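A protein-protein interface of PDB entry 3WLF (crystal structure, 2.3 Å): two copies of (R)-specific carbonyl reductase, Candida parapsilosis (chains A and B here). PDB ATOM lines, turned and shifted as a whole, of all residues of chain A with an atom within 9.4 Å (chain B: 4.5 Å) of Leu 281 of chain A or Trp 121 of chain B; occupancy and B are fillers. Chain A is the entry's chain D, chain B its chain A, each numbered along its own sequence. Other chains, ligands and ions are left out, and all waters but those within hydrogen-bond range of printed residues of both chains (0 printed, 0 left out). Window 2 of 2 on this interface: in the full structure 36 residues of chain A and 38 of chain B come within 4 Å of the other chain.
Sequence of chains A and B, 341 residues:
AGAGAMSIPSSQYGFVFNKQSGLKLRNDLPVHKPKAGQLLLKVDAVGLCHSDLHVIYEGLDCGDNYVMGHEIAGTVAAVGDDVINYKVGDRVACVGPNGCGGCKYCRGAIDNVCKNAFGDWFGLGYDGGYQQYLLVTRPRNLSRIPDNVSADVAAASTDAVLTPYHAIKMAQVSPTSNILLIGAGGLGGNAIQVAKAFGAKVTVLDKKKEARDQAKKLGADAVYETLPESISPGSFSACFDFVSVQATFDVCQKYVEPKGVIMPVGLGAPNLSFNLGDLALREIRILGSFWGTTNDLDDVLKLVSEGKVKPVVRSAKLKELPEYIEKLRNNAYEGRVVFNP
The backbone NH (N) of Phe 290 of chain B sits at hydrogen-bond distance from the side-chain carboxylate (OE2) of Glu 283 of chain A, 3.1 Å away.
The side-chain amino group of Lys 259 of chain A lies within salt-bridge range of the side-chain carboxylate of Glu 283 of chain A, 3.7 Å away.
The backbone carbonyl oxygen (O) of Trp 121 of chain B sits at hydrogen-bond distance from the backbone NH (N) of Tyr 126 of chain B, at 2.9 Å.
Ala 280 of chain A touches Phe 290 of chain B.
Val 113 of chain B touches Leu 281 of chain A.
Leu 281 of chain A touches Phe 118 of chain B.
Leu 281 of chain A touches Trp 121 of chain B (CD1 to CH2, 3.9 Å).
Leu 281 of chain A touches Phe 290 of chain B (O to CB, 3.8 Å).
CG of Glu 283 of chain A touches CG1 of Val 113 of chain B (3.6 Å).
Leu 281 of chain A touches just these residues of chain B: Val 113, Phe 118, Trp 121 and Phe 290.
Of chain A, only Leu 281 comes within 4 Å of Trp 121 of chain B.
No residue of chain A comes within 4 Å of Gly 119 of chain B.
No residue of chain A comes within 4 Å of Asp 120 of chain B.
Gly 123 of chain B touches none of the printed residues of chain A.
Printed residues of chain A within 4 Å of Phe 118 of chain B: Leu 281.
Printed residues of chain A within 4 Å of Val 113 of chain B: Leu 281 (3.8 Å) and Glu 283 (3.6 Å).
Printed residues of chain A within 4 Å of Phe 290 of chain B: Ala 280 (3.2 Å), Leu 281 (3.8 Å) and Glu 283 (3.1 Å).
Of the printed residues of chain B, Ala 280 of chain A touches Phe 290.
Printed residues of chain B within 4 Å of Glu 283 of chain A: Val 113 and Phe 290.
The nearest printed residue of chain B that does not touch Leu 281 of chain A is Trp 291 of chain B (7.1 Å).
The nearest residue of chain A that does not touch Trp 121 of chain B is Arg 282 of chain A (8.4 Å).
The nearest printed residue of chain B that does not touch Ala 280 of chain A is Val 113 of chain B (5.8 Å).
Printed residues of chain B that touch a printed residue of chain A: Val 113, Phe 118, Trp 121 and Phe 290.
Hydrophobic or aromatic side chains of chain B that line the printed part of chain A: Val 113, Phe 118, Trp 121 and Phe 290.
Among the printed residues, no Asp or Glu carboxylate lies within 4 Å of a Lys or Arg side-chain nitrogen of the other chain.
No position is printed for both chains.
Of the 7 pairs that touch across the chains among the printed residues, none has its exchanged pair printed and touching as well.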
ATOM      1  N   GLN A 253      -8.428   8.805  16.926  1.00  0.00           N
ATOM      2  CA  GLN A 253      -8.733  10.224  16.777  1.00  0.00           C
ATOM      3  C   GLN A 253      -9.840  10.444  15.759  1.00  0.00           C
ATOM      4  O   GLN A 253     -10.592  11.415  15.842  1.00  0.00           O
ATOM      5  CB  GLN A 253      -7.482  11.007  16.361  1.00  0.00           C
ATOM      6  CG  GLN A 253      -7.776  12.421  15.881  1.00  0.00           C
ATOM      7  CD  GLN A 253      -6.571  13.335  15.956  1.00  0.00           C
ATOM      8  OE1 GLN A 253      -5.479  12.983  15.514  1.00  0.00           O
ATOM      9  NE2 GLN A 253      -6.770  14.525  16.512  1.00  0.00           N
ATOM     10  N   GLU A 257     -15.450  10.650  19.732  1.00  0.00           N
ATOM     11  CA  GLU A 257     -16.401  11.755  19.680  1.00  0.00           C
ATOM     12  C   GLU A 257     -15.804  13.005  20.323  1.00  0.00           C
ATOM     13  O   GLU A 257     -14.789  12.932  21.017  1.00  0.00           O
ATOM     14  CB  GLU A 257     -17.698  11.374  20.402  1.00  0.00           C
ATOM     15  CG  GLU A 257     -17.578  11.310  21.920  1.00  0.00           C
ATOM     16  CD  GLU A 257     -18.882  10.922  22.600  1.00  0.00           C
ATOM     17  OE1 GLU A 257     -18.950  10.995  23.844  1.00  0.00           O
ATOM     18  OE2 GLU A 257     -19.836  10.539  21.893  1.00  0.00           O
ATOM     19  N   PRO A 258     -16.426  14.173  20.096  1.00  0.00           N
ATOM     20  CA  PRO A 258     -15.930  15.425  20.675  1.00  0.00           C
ATOM     21  C   PRO A 258     -15.802  15.320  22.191  1.00  0.00           C
ATOM     22  O   PRO A 258     -16.689  14.789  22.860  1.00  0.00           O
ATOM     23  CB  PRO A 258     -16.984  16.440  20.250  1.00  0.00           C
ATOM     24  CG  PRO A 258     -17.418  15.912  18.915  1.00  0.00           C
ATOM     25  CD  PRO A 258     -17.565  14.433  19.197  1.00  0.00           C
ATOM     26  N   LYS A 259     -14.692  15.826  22.718  1.00  0.00           N
ATOM     27  CA  LYS A 259     -14.418  15.799  24.149  1.00  0.00           C
ATOM     28  C   LYS A 259     -14.209  14.364  24.626  1.00  0.00           C
ATOM     29  O   LYS A 259     -14.227  14.085  25.824  1.00  0.00           O
ATOM     30  CB  LYS A 259     -15.569  16.455  24.921  1.00  0.00           C
ATOM     31  CG  LYS A 259     -15.192  16.935  26.314  1.00  0.00           C
ATOM     32  CD  LYS A 259     -14.013  17.893  26.251  1.00  0.00           C
ATOM     33  CE  LYS A 259     -13.677  18.470  27.616  1.00  0.00           C
ATOM     34  NZ  LYS A 259     -14.761  19.350  28.124  1.00  0.00           N
ATOM     35  N   GLY A 260     -14.006  13.457  23.674  1.00  0.00           N
ATOM     36  CA  GLY A 260     -13.783  12.062  24.006  1.00  0.00           C
ATOM     37  C   GLY A 260     -12.342  11.844  24.416  1.00  0.00           C
ATOM     38  O   GLY A 260     -11.529  12.763  24.330  1.00  0.00           O
ATOM     39  N   ASN A 275      -3.379  15.064  15.072  1.00  0.00           N
ATOM     40  CA  ASN A 275      -3.760  16.257  14.333  1.00  0.00           C
ATOM     41  C   ASN A 275      -4.126  17.336  15.350  1.00  0.00           C
ATOM     42  O   ASN A 275      -5.094  17.192  16.099  1.00  0.00           O
ATOM     43  CB  ASN A 275      -4.952  15.956  13.425  1.00  0.00           C
ATOM     44  CG  ASN A 275      -5.337  17.137  12.561  1.00  0.00           C
ATOM     45  OD1 ASN A 275      -5.662  18.211  13.066  1.00  0.00           O
ATOM     46  ND2 ASN A 275      -5.307  16.944  11.247  1.00  0.00           N
ATOM     47  N   LEU A 276      -3.344  18.412  15.375  1.00  0.00           N
ATOM     48  CA  LEU A 276      -3.568  19.510  16.308  1.00  0.00           C
ATOM     49  C   LEU A 276      -4.903  20.214  16.091  1.00  0.00           C
ATOM     50  O   LEU A 276      -5.632  20.484  17.044  1.00  0.00           O
ATOM     51  CB  LEU A 276      -2.429  20.529  16.203  1.00  0.00           C
ATOM     52  CG  LEU A 276      -2.463  21.691  17.201  1.00  0.00           C
ATOM     53  CD1 LEU A 276      -2.439  21.150  18.628  1.00  0.00           C
ATOM     54  CD2 LEU A 276      -1.275  22.611  16.957  1.00  0.00           C
ATOM     55  N   GLY A 277      -5.220  20.512  14.836  1.00  0.00           N
ATOM     56  CA  GLY A 277      -6.468  21.186  14.533  1.00  0.00           C
ATOM     57  C   GLY A 277      -7.690  20.425  15.011  1.00  0.00           C
ATOM     58  O   GLY A 277      -8.609  21.007  15.590  1.00  0.00           O
ATOM     59  N   ASP A 278      -7.703  19.119  14.774  1.00  0.00           N
ATOM     60  CA  ASP A 278      -8.825  18.280  15.172  1.00  0.00           C
ATOM     61  C   ASP A 278      -8.922  18.139  16.688  1.00  0.00           C
ATOM     62  O   ASP A 278      -9.993  18.305  17.272  1.00  0.00           O
ATOM     63  CB  ASP A 278      -8.692  16.893  14.544  1.00  0.00           C
ATOM     64  CG  ASP A 278      -9.867  15.998  14.869  1.00  0.00           C
ATOM     65  OD1 ASP A 278     -10.979  16.274  14.370  1.00  0.00           O
ATOM     66  OD2 ASP A 278      -9.681  15.025  15.630  1.00  0.00           O
ATOM     67  N   LEU A 279      -7.795  17.828  17.320  1.00  0.00           N
ATOM     68  CA  LEU A 279      -7.753  17.656  18.766  1.00  0.00           C
ATOM     69  C   LEU A 279      -8.219  18.905  19.507  1.00  0.00           C
ATOM     70  O   LEU A 279      -8.898  18.809  20.528  1.00  0.00           O
ATOM     71  CB  LEU A 279      -6.334  17.282  19.208  1.00  0.00           C
ATOM     72  CG  LEU A 279      -6.055  17.226  20.713  1.00  0.00           C
ATOM     73  CD1 LEU A 279      -5.044  16.132  21.012  1.00  0.00           C
ATOM     74  CD2 LEU A 279      -5.547  18.579  21.190  1.00  0.00           C
ATOM     75  N   ALA A 280      -7.858  20.072  18.983  1.00  0.00           N
ATOM     76  CA  ALA A 280      -8.235  21.337  19.599  1.00  0.00           C
ATOM     77  C   ALA A 280      -9.696  21.684  19.342  1.00  0.00           C
ATOM     78  O   ALA A 280     -10.426  22.057  20.262  1.00  0.00           O
ATOM     79  CB  ALA A 280      -7.333  22.454  19.080  1.00  0.00           C
ATOM     80  N   LEU A 281     -10.120  21.553  18.088  1.00  0.00           N
ATOM     81  CA  LEU A 281     -11.487  21.867  17.691  1.00  0.00           C
ATOM     82  C   LEU A 281     -12.541  21.005  18.378  1.00  0.00           C
ATOM     83  O   LEU A 281     -13.579  21.508  18.807  1.00  0.00           O
ATOM     84  CB  LEU A 281     -11.636  21.727  16.173  1.00  0.00           C
ATOM     85  CG  LEU A 281     -13.029  22.002  15.595  1.00  0.00           C
ATOM     86  CD1 LEU A 281     -13.411  23.456  15.839  1.00  0.00           C
ATOM     87  CD2 LEU A 281     -13.038  21.692  14.106  1.00  0.00           C
ATOM     88  N   ARG A 282     -12.280  19.708  18.476  1.00  0.00           N
ATOM     89  CA  ARG A 282     -13.233  18.798  19.099  1.00  0.00           C
ATOM     90  C   ARG A 282     -12.836  18.435  20.527  1.00  0.00           C
ATOM     91  O   ARG A 282     -13.344  17.474  21.102  1.00  0.00           O
ATOM     92  CB  ARG A 282     -13.381  17.542  18.236  1.00  0.00           C
ATOM     93  CG  ARG A 282     -13.811  17.855  16.805  1.00  0.00           C
ATOM     94  CD  ARG A 282     -14.145  16.599  16.022  1.00  0.00           C
ATOM     95  NE  ARG A 282     -13.021  15.672  15.977  1.00  0.00           N
ATOM     96  CZ  ARG A 282     -13.086  14.404  16.368  1.00  0.00           C
ATOM     97  NH1 ARG A 282     -12.013  13.631  16.291  1.00  0.00           N
ATOM     98  NH2 ARG A 282     -14.226  13.909  16.834  1.00  0.00           N
ATOM     99  N   GLU A 283     -11.928  19.226  21.088  1.00  0.00           N
ATOM    100  CA  GLU A 283     -11.442  19.043  22.450  1.00  0.00           C
ATOM    101  C   GLU A 283     -11.175  17.596  22.835  1.00  0.00           C
ATOM    102  O   GLU A 283     -11.558  17.146  23.917  1.00  0.00           O
ATOM    103  CB  GLU A 283     -12.426  19.660  23.446  1.00  0.00           C
ATOM    104  CG  GLU A 283     -12.768  21.107  23.145  1.00  0.00           C
ATOM    105  CD  GLU A 283     -13.315  21.842  24.353  1.00  0.00           C
ATOM    106  OE1 GLU A 283     -14.216  21.307  25.036  1.00  0.00           O
ATOM    107  OE2 GLU A 283     -12.840  22.966  24.612  1.00  0.00           O
ATOM    108  N   ILE A 284     -10.520  16.868  21.941  1.00  0.00           N
ATOM    109  CA  ILE A 284     -10.177  15.481  22.200  1.00  0.00           C
ATOM    110  C   ILE A 284      -9.069  15.476  23.244  1.00  0.00           C
ATOM    111  O   ILE A 284      -8.241  16.384  23.282  1.00  0.00           O
ATOM    112  CB  ILE A 284      -9.661  14.790  20.926  1.00  0.00           C
ATOM    113  CG1 ILE A 284     -10.753  14.808  19.857  1.00  0.00           C
ATOM    114  CG2 ILE A 284      -9.239  13.362  21.237  1.00  0.00           C
ATOM    115  CD1 ILE A 284     -10.313  14.227  18.543  1.00  0.00           C
ATOM    116  N   ARG A 285      -9.059  14.463  24.099  1.00  0.00           N
ATOM    117  CA  ARG A 285      -8.032  14.376  25.120  1.00  0.00           C
ATOM    118  C   ARG A 285      -7.310  13.039  25.113  1.00  0.00           C
ATOM    119  O   ARG A 285      -7.926  11.978  25.034  1.00  0.00           O
ATOM    120  CB  ARG A 285      -8.628  14.664  26.502  1.00  0.00           C
ATOM    121  CG  ARG A 285      -9.963  14.006  26.779  1.00  0.00           C
ATOM    122  CD  ARG A 285     -10.704  14.768  27.871  1.00  0.00           C
ATOM    123  NE  ARG A 285     -12.047  14.241  28.092  1.00  0.00           N
ATOM    124  CZ  ARG A 285     -12.308  13.073  28.670  1.00  0.00           C
ATOM    125  NH1 ARG A 285     -11.316  12.301  29.092  1.00  0.00           N
ATOM    126  NH2 ARG A 285     -13.563  12.672  28.818  1.00  0.00           N
ATOM    127  N   GLY B  96     -19.560  33.144  20.525  1.00  0.00           N
ATOM    128  CA  GLY B  96     -19.145  32.669  19.213  1.00  0.00           C
ATOM    129  C   GLY B  96     -19.690  31.353  18.684  1.00  0.00           C
ATOM    130  O   GLY B  96     -20.436  31.355  17.707  1.00  0.00           O
ATOM    131  N   PRO B  97     -19.327  30.211  19.292  1.00  0.00           N
ATOM    132  CA  PRO B  97     -19.787  28.883  18.866  1.00  0.00           C
ATOM    133  C   PRO B  97     -21.281  28.790  18.555  1.00  0.00           C
ATOM    134  O   PRO B  97     -21.703  27.942  17.766  1.00  0.00           O
ATOM    135  CB  PRO B  97     -19.369  27.992  20.029  1.00  0.00           C
ATOM    136  CG  PRO B  97     -18.075  28.619  20.447  1.00  0.00           C
ATOM    137  CD  PRO B  97     -18.422  30.097  20.451  1.00  0.00           C
ATOM    138  N   ASN B  98     -22.074  29.652  19.185  1.00  0.00           N
ATOM    139  CA  ASN B  98     -23.516  29.693  18.951  1.00  0.00           C
ATOM    140  C   ASN B  98     -24.146  28.296  18.864  1.00  0.00           C
ATOM    141  O   ASN B  98     -24.802  27.964  17.880  1.00  0.00           O
ATOM    142  CB  ASN B  98     -23.779  30.479  17.660  1.00  0.00           C
ATOM    143  CG  ASN B  98     -25.250  30.775  17.436  1.00  0.00           C
ATOM    144  OD1 ASN B  98     -25.953  31.217  18.344  1.00  0.00           O
ATOM    145  ND2 ASN B  98     -25.718  30.551  16.212  1.00  0.00           N
ATOM    146  N   VAL B 113     -18.511  22.731  21.432  1.00  0.00           N
ATOM    147  CA  VAL B 113     -18.159  21.689  20.471  1.00  0.00           C
ATOM    148  C   VAL B 113     -19.414  21.082  19.849  1.00  0.00           C
ATOM    149  O   VAL B 113     -19.429  19.911  19.467  1.00  0.00           O
ATOM    150  CB  VAL B 113     -17.328  20.556  21.124  1.00  0.00           C
ATOM    151  CG1 VAL B 113     -16.022  21.115  21.663  1.00  0.00           C
ATOM    152  CG2 VAL B 113     -18.122  19.890  22.233  1.00  0.00           C
ATOM    153  N   ALA B 117     -24.132  23.205  15.392  1.00  0.00           N
ATOM    154  CA  ALA B 117     -23.786  24.615  15.251  1.00  0.00           C
ATOM    155  C   ALA B 117     -22.604  24.816  14.308  1.00  0.00           C
ATOM    156  O   ALA B 117     -22.236  25.947  13.992  1.00  0.00           O
ATOM    157  CB  ALA B 117     -23.472  25.214  16.619  1.00  0.00           C
ATOM    158  N   PHE B 118     -22.012  23.714  13.860  1.00  0.00           N
ATOM    159  CA  PHE B 118     -20.875  23.788  12.954  1.00  0.00           C
ATOM    160  C   PHE B 118     -21.292  24.511  11.676  1.00  0.00           C
ATOM    161  O   PHE B 118     -22.253  24.118  11.016  1.00  0.00           O
ATOM    162  CB  PHE B 118     -20.373  22.381  12.622  1.00  0.00           C
ATOM    163  CG  PHE B 118     -18.878  22.270  12.583  1.00  0.00           C
ATOM    164  CD1 PHE B 118     -18.135  23.001  11.663  1.00  0.00           C
ATOM    165  CD2 PHE B 118     -18.210  21.447  13.483  1.00  0.00           C
ATOM    166  CE1 PHE B 118     -16.745  22.919  11.640  1.00  0.00           C
ATOM    167  CE2 PHE B 118     -16.821  21.356  13.470  1.00  0.00           C
ATOM    168  CZ  PHE B 118     -16.087  22.094  12.547  1.00  0.00           C
ATOM    169  N   GLY B 119     -20.568  25.573  11.339  1.00  0.00           N
ATOM    170  CA  GLY B 119     -20.888  26.343  10.152  1.00  0.00           C
ATOM    171  C   GLY B 119     -21.974  27.363  10.443  1.00  0.00           C
ATOM    172  O   GLY B 119     -22.505  28.001   9.534  1.00  0.00           O
ATOM    173  N   ASP B 120     -22.302  27.524  11.722  1.00  0.00           N
ATOM    174  CA  ASP B 120     -23.338  28.463  12.125  1.00  0.00           C
ATOM    175  C   ASP B 120     -22.861  29.377  13.252  1.00  0.00           C
ATOM    176  O   ASP B 120     -23.672  29.945  13.982  1.00  0.00           O
ATOM    177  CB  ASP B 120     -24.590  27.697  12.566  1.00  0.00           C
ATOM    178  CG  ASP B 120     -25.822  28.580  12.642  1.00  0.00           C
ATOM    179  OD1 ASP B 120     -26.184  29.190  11.613  1.00  0.00           O
ATOM    180  OD2 ASP B 120     -26.431  28.660  13.730  1.00  0.00           O
ATOM    181  N   TRP B 121     -21.545  29.515  13.390  1.00  0.00           N
ATOM    182  CA  TRP B 121     -20.979  30.374  14.426  1.00  0.00           C
ATOM    183  C   TRP B 121     -21.189  31.839  14.059  1.00  0.00           C
ATOM    184  O   TRP B 121     -21.315  32.180  12.882  1.00  0.00           O
ATOM    185  CB  TRP B 121     -19.472  30.136  14.586  1.00  0.00           C
ATOM    186  CG  TRP B 121     -19.065  28.727  14.892  1.00  0.00           C
ATOM    187  CD1 TRP B 121     -19.809  27.769  15.521  1.00  0.00           C
ATOM    188  CD2 TRP B 121     -17.784  28.138  14.639  1.00  0.00           C
ATOM    189  NE1 TRP B 121     -19.069  26.619  15.677  1.00  0.00           N
ATOM    190  CE2 TRP B 121     -17.823  26.819  15.145  1.00  0.00           C
ATOM    191  CE3 TRP B 121     -16.604  28.597  14.035  1.00  0.00           C
ATOM    192  CZ2 TRP B 121     -16.726  25.954  15.066  1.00  0.00           C
ATOM    193  CZ3 TRP B 121     -15.514  27.737  13.956  1.00  0.00           C
ATOM    194  CH2 TRP B 121     -15.584  26.429  14.470  1.00  0.00           C
ATOM    195  N   PHE B 122     -21.214  32.703  15.070  1.00  0.00           N
ATOM    196  CA  PHE B 122     -21.390  34.134  14.847  1.00  0.00           C
ATOM    197  C   PHE B 122     -20.231  34.694  14.023  1.00  0.00           C
ATOM    198  O   PHE B 122     -19.068  34.527  14.385  1.00  0.00           O
ATOM    199  CB  PHE B 122     -21.467  34.874  16.186  1.00  0.00           C
ATOM    200  CG  PHE B 122     -22.785  34.721  16.893  1.00  0.00           C
ATOM    201  CD1 PHE B 122     -23.943  35.278  16.360  1.00  0.00           C
ATOM    202  CD2 PHE B 122     -22.867  34.027  18.096  1.00  0.00           C
ATOM    203  CE1 PHE B 122     -25.168  35.149  17.015  1.00  0.00           C
ATOM    204  CE2 PHE B 122     -24.087  33.891  18.761  1.00  0.00           C
ATOM    205  CZ  PHE B 122     -25.240  34.453  18.217  1.00  0.00           C
ATOM    206  N   GLY B 123     -20.557  35.353  12.915  1.00  0.00           N
ATOM    207  CA  GLY B 123     -19.530  35.932  12.062  1.00  0.00           C
ATOM    208  C   GLY B 123     -18.647  34.911  11.365  1.00  0.00           C
ATOM    209  O   GLY B 123     -17.752  35.276  10.603  1.00  0.00           O
ATOM    210  N   LEU B 124     -18.900  33.632  11.621  1.00  0.00           N
ATOM    211  CA  LEU B 124     -18.123  32.554  11.017  1.00  0.00           C
ATOM    212  C   LEU B 124     -19.052  31.426  10.581  1.00  0.00           C
ATOM    213  O   LEU B 124     -18.981  30.308  11.095  1.00  0.00           O
ATOM    214  CB  LEU B 124     -17.093  32.035  12.023  1.00  0.00           C
ATOM    215  CG  LEU B 124     -16.025  33.054  12.430  1.00  0.00           C
ATOM    216  CD1 LEU B 124     -15.230  32.544  13.621  1.00  0.00           C
ATOM    217  CD2 LEU B 124     -15.113  33.319  11.244  1.00  0.00           C
ATOM    218  N   GLY B 125     -19.921  31.735   9.624  1.00  0.00           N
ATOM    219  CA  GLY B 125     -20.880  30.762   9.133  1.00  0.00           C
ATOM    220  C   GLY B 125     -22.252  31.403   9.184  1.00  0.00           C
ATOM    221  O   GLY B 125     -23.049  31.290   8.254  1.00  0.00           O
ATOM    222  N   TYR B 126     -22.523  32.079  10.296  1.00  0.00           N
ATOM    223  CA  TYR B 126     -23.781  32.783  10.489  1.00  0.00           C
ATOM    224  C   TYR B 126     -23.425  34.260  10.590  1.00  0.00           C
ATOM    225  O   TYR B 126     -22.287  34.600  10.908  1.00  0.00           O
ATOM    226  CB  TYR B 126     -24.472  32.318  11.774  1.00  0.00           C
ATOM    227  CG  TYR B 126     -25.774  33.035  12.048  1.00  0.00           C
ATOM    228  CD1 TYR B 126     -26.824  32.987  11.129  1.00  0.00           C
ATOM    229  CD2 TYR B 126     -25.948  33.791  13.205  1.00  0.00           C
ATOM    230  CE1 TYR B 126     -28.011  33.678  11.355  1.00  0.00           C
ATOM    231  CE2 TYR B 126     -27.132  34.486  13.440  1.00  0.00           C
ATOM    232  CZ  TYR B 126     -28.157  34.425  12.510  1.00  0.00           C
ATOM    233  OH  TYR B 126     -29.325  35.118  12.731  1.00  0.00           O
ATOM    234  N   PHE B 290     -11.000  24.643  22.714  1.00  0.00           N
ATOM    235  CA  PHE B 290     -11.559  25.480  21.656  1.00  0.00           C
ATOM    236  C   PHE B 290     -12.471  26.583  22.183  1.00  0.00           C
ATOM    237  O   PHE B 290     -13.436  26.316  22.901  1.00  0.00           O
ATOM    238  CB  PHE B 290     -12.336  24.622  20.656  1.00  0.00           C
ATOM    239  CG  PHE B 290     -13.012  25.416  19.571  1.00  0.00           C
ATOM    240  CD1 PHE B 290     -12.266  26.206  18.703  1.00  0.00           C
ATOM    241  CD2 PHE B 290     -14.393  25.383  19.426  1.00  0.00           C
ATOM    242  CE1 PHE B 290     -12.890  26.955  17.705  1.00  0.00           C
ATOM    243  CE2 PHE B 290     -15.027  26.127  18.432  1.00  0.00           C
ATOM    244  CZ  PHE B 290     -14.274  26.914  17.570  1.00  0.00           C
ATOM    245  N   TRP B 291     -12.158  27.821  21.811  1.00  0.00           N
ATOM    246  CA  TRP B 291     -12.941  28.985  22.220  1.00  0.00           C
ATOM    247  C   TRP B 291     -13.371  28.887  23.682  1.00  0.00           C
ATOM    248  O   TRP B 291     -12.545  28.679  24.573  1.00  0.00           O
ATOM    249  CB  TRP B 291     -14.183  29.116  21.332  1.00  0.00           C
ATOM    250  CG  TRP B 291     -14.512  30.526  20.936  1.00  0.00           C
ATOM    251  CD1 TRP B 291     -14.385  31.647  21.705  1.00  0.00           C
ATOM    252  CD2 TRP B 291     -15.052  30.960  19.682  1.00  0.00           C
ATOM    253  NE1 TRP B 291     -14.812  32.753  21.008  1.00  0.00           N
ATOM    254  CE2 TRP B 291     -15.227  32.359  19.765  1.00  0.00           C
ATOM    255  CE3 TRP B 291     -15.407  30.301  18.497  1.00  0.00           C
ATOM    256  CZ2 TRP B 291     -15.742  33.113  18.704  1.00  0.00           C
ATOM    257  CZ3 TRP B 291     -15.919  31.053  17.441  1.00  0.00           C
ATOM    258  CH2 TRP B 291     -16.081  32.445  17.555  1.00  0.00           C
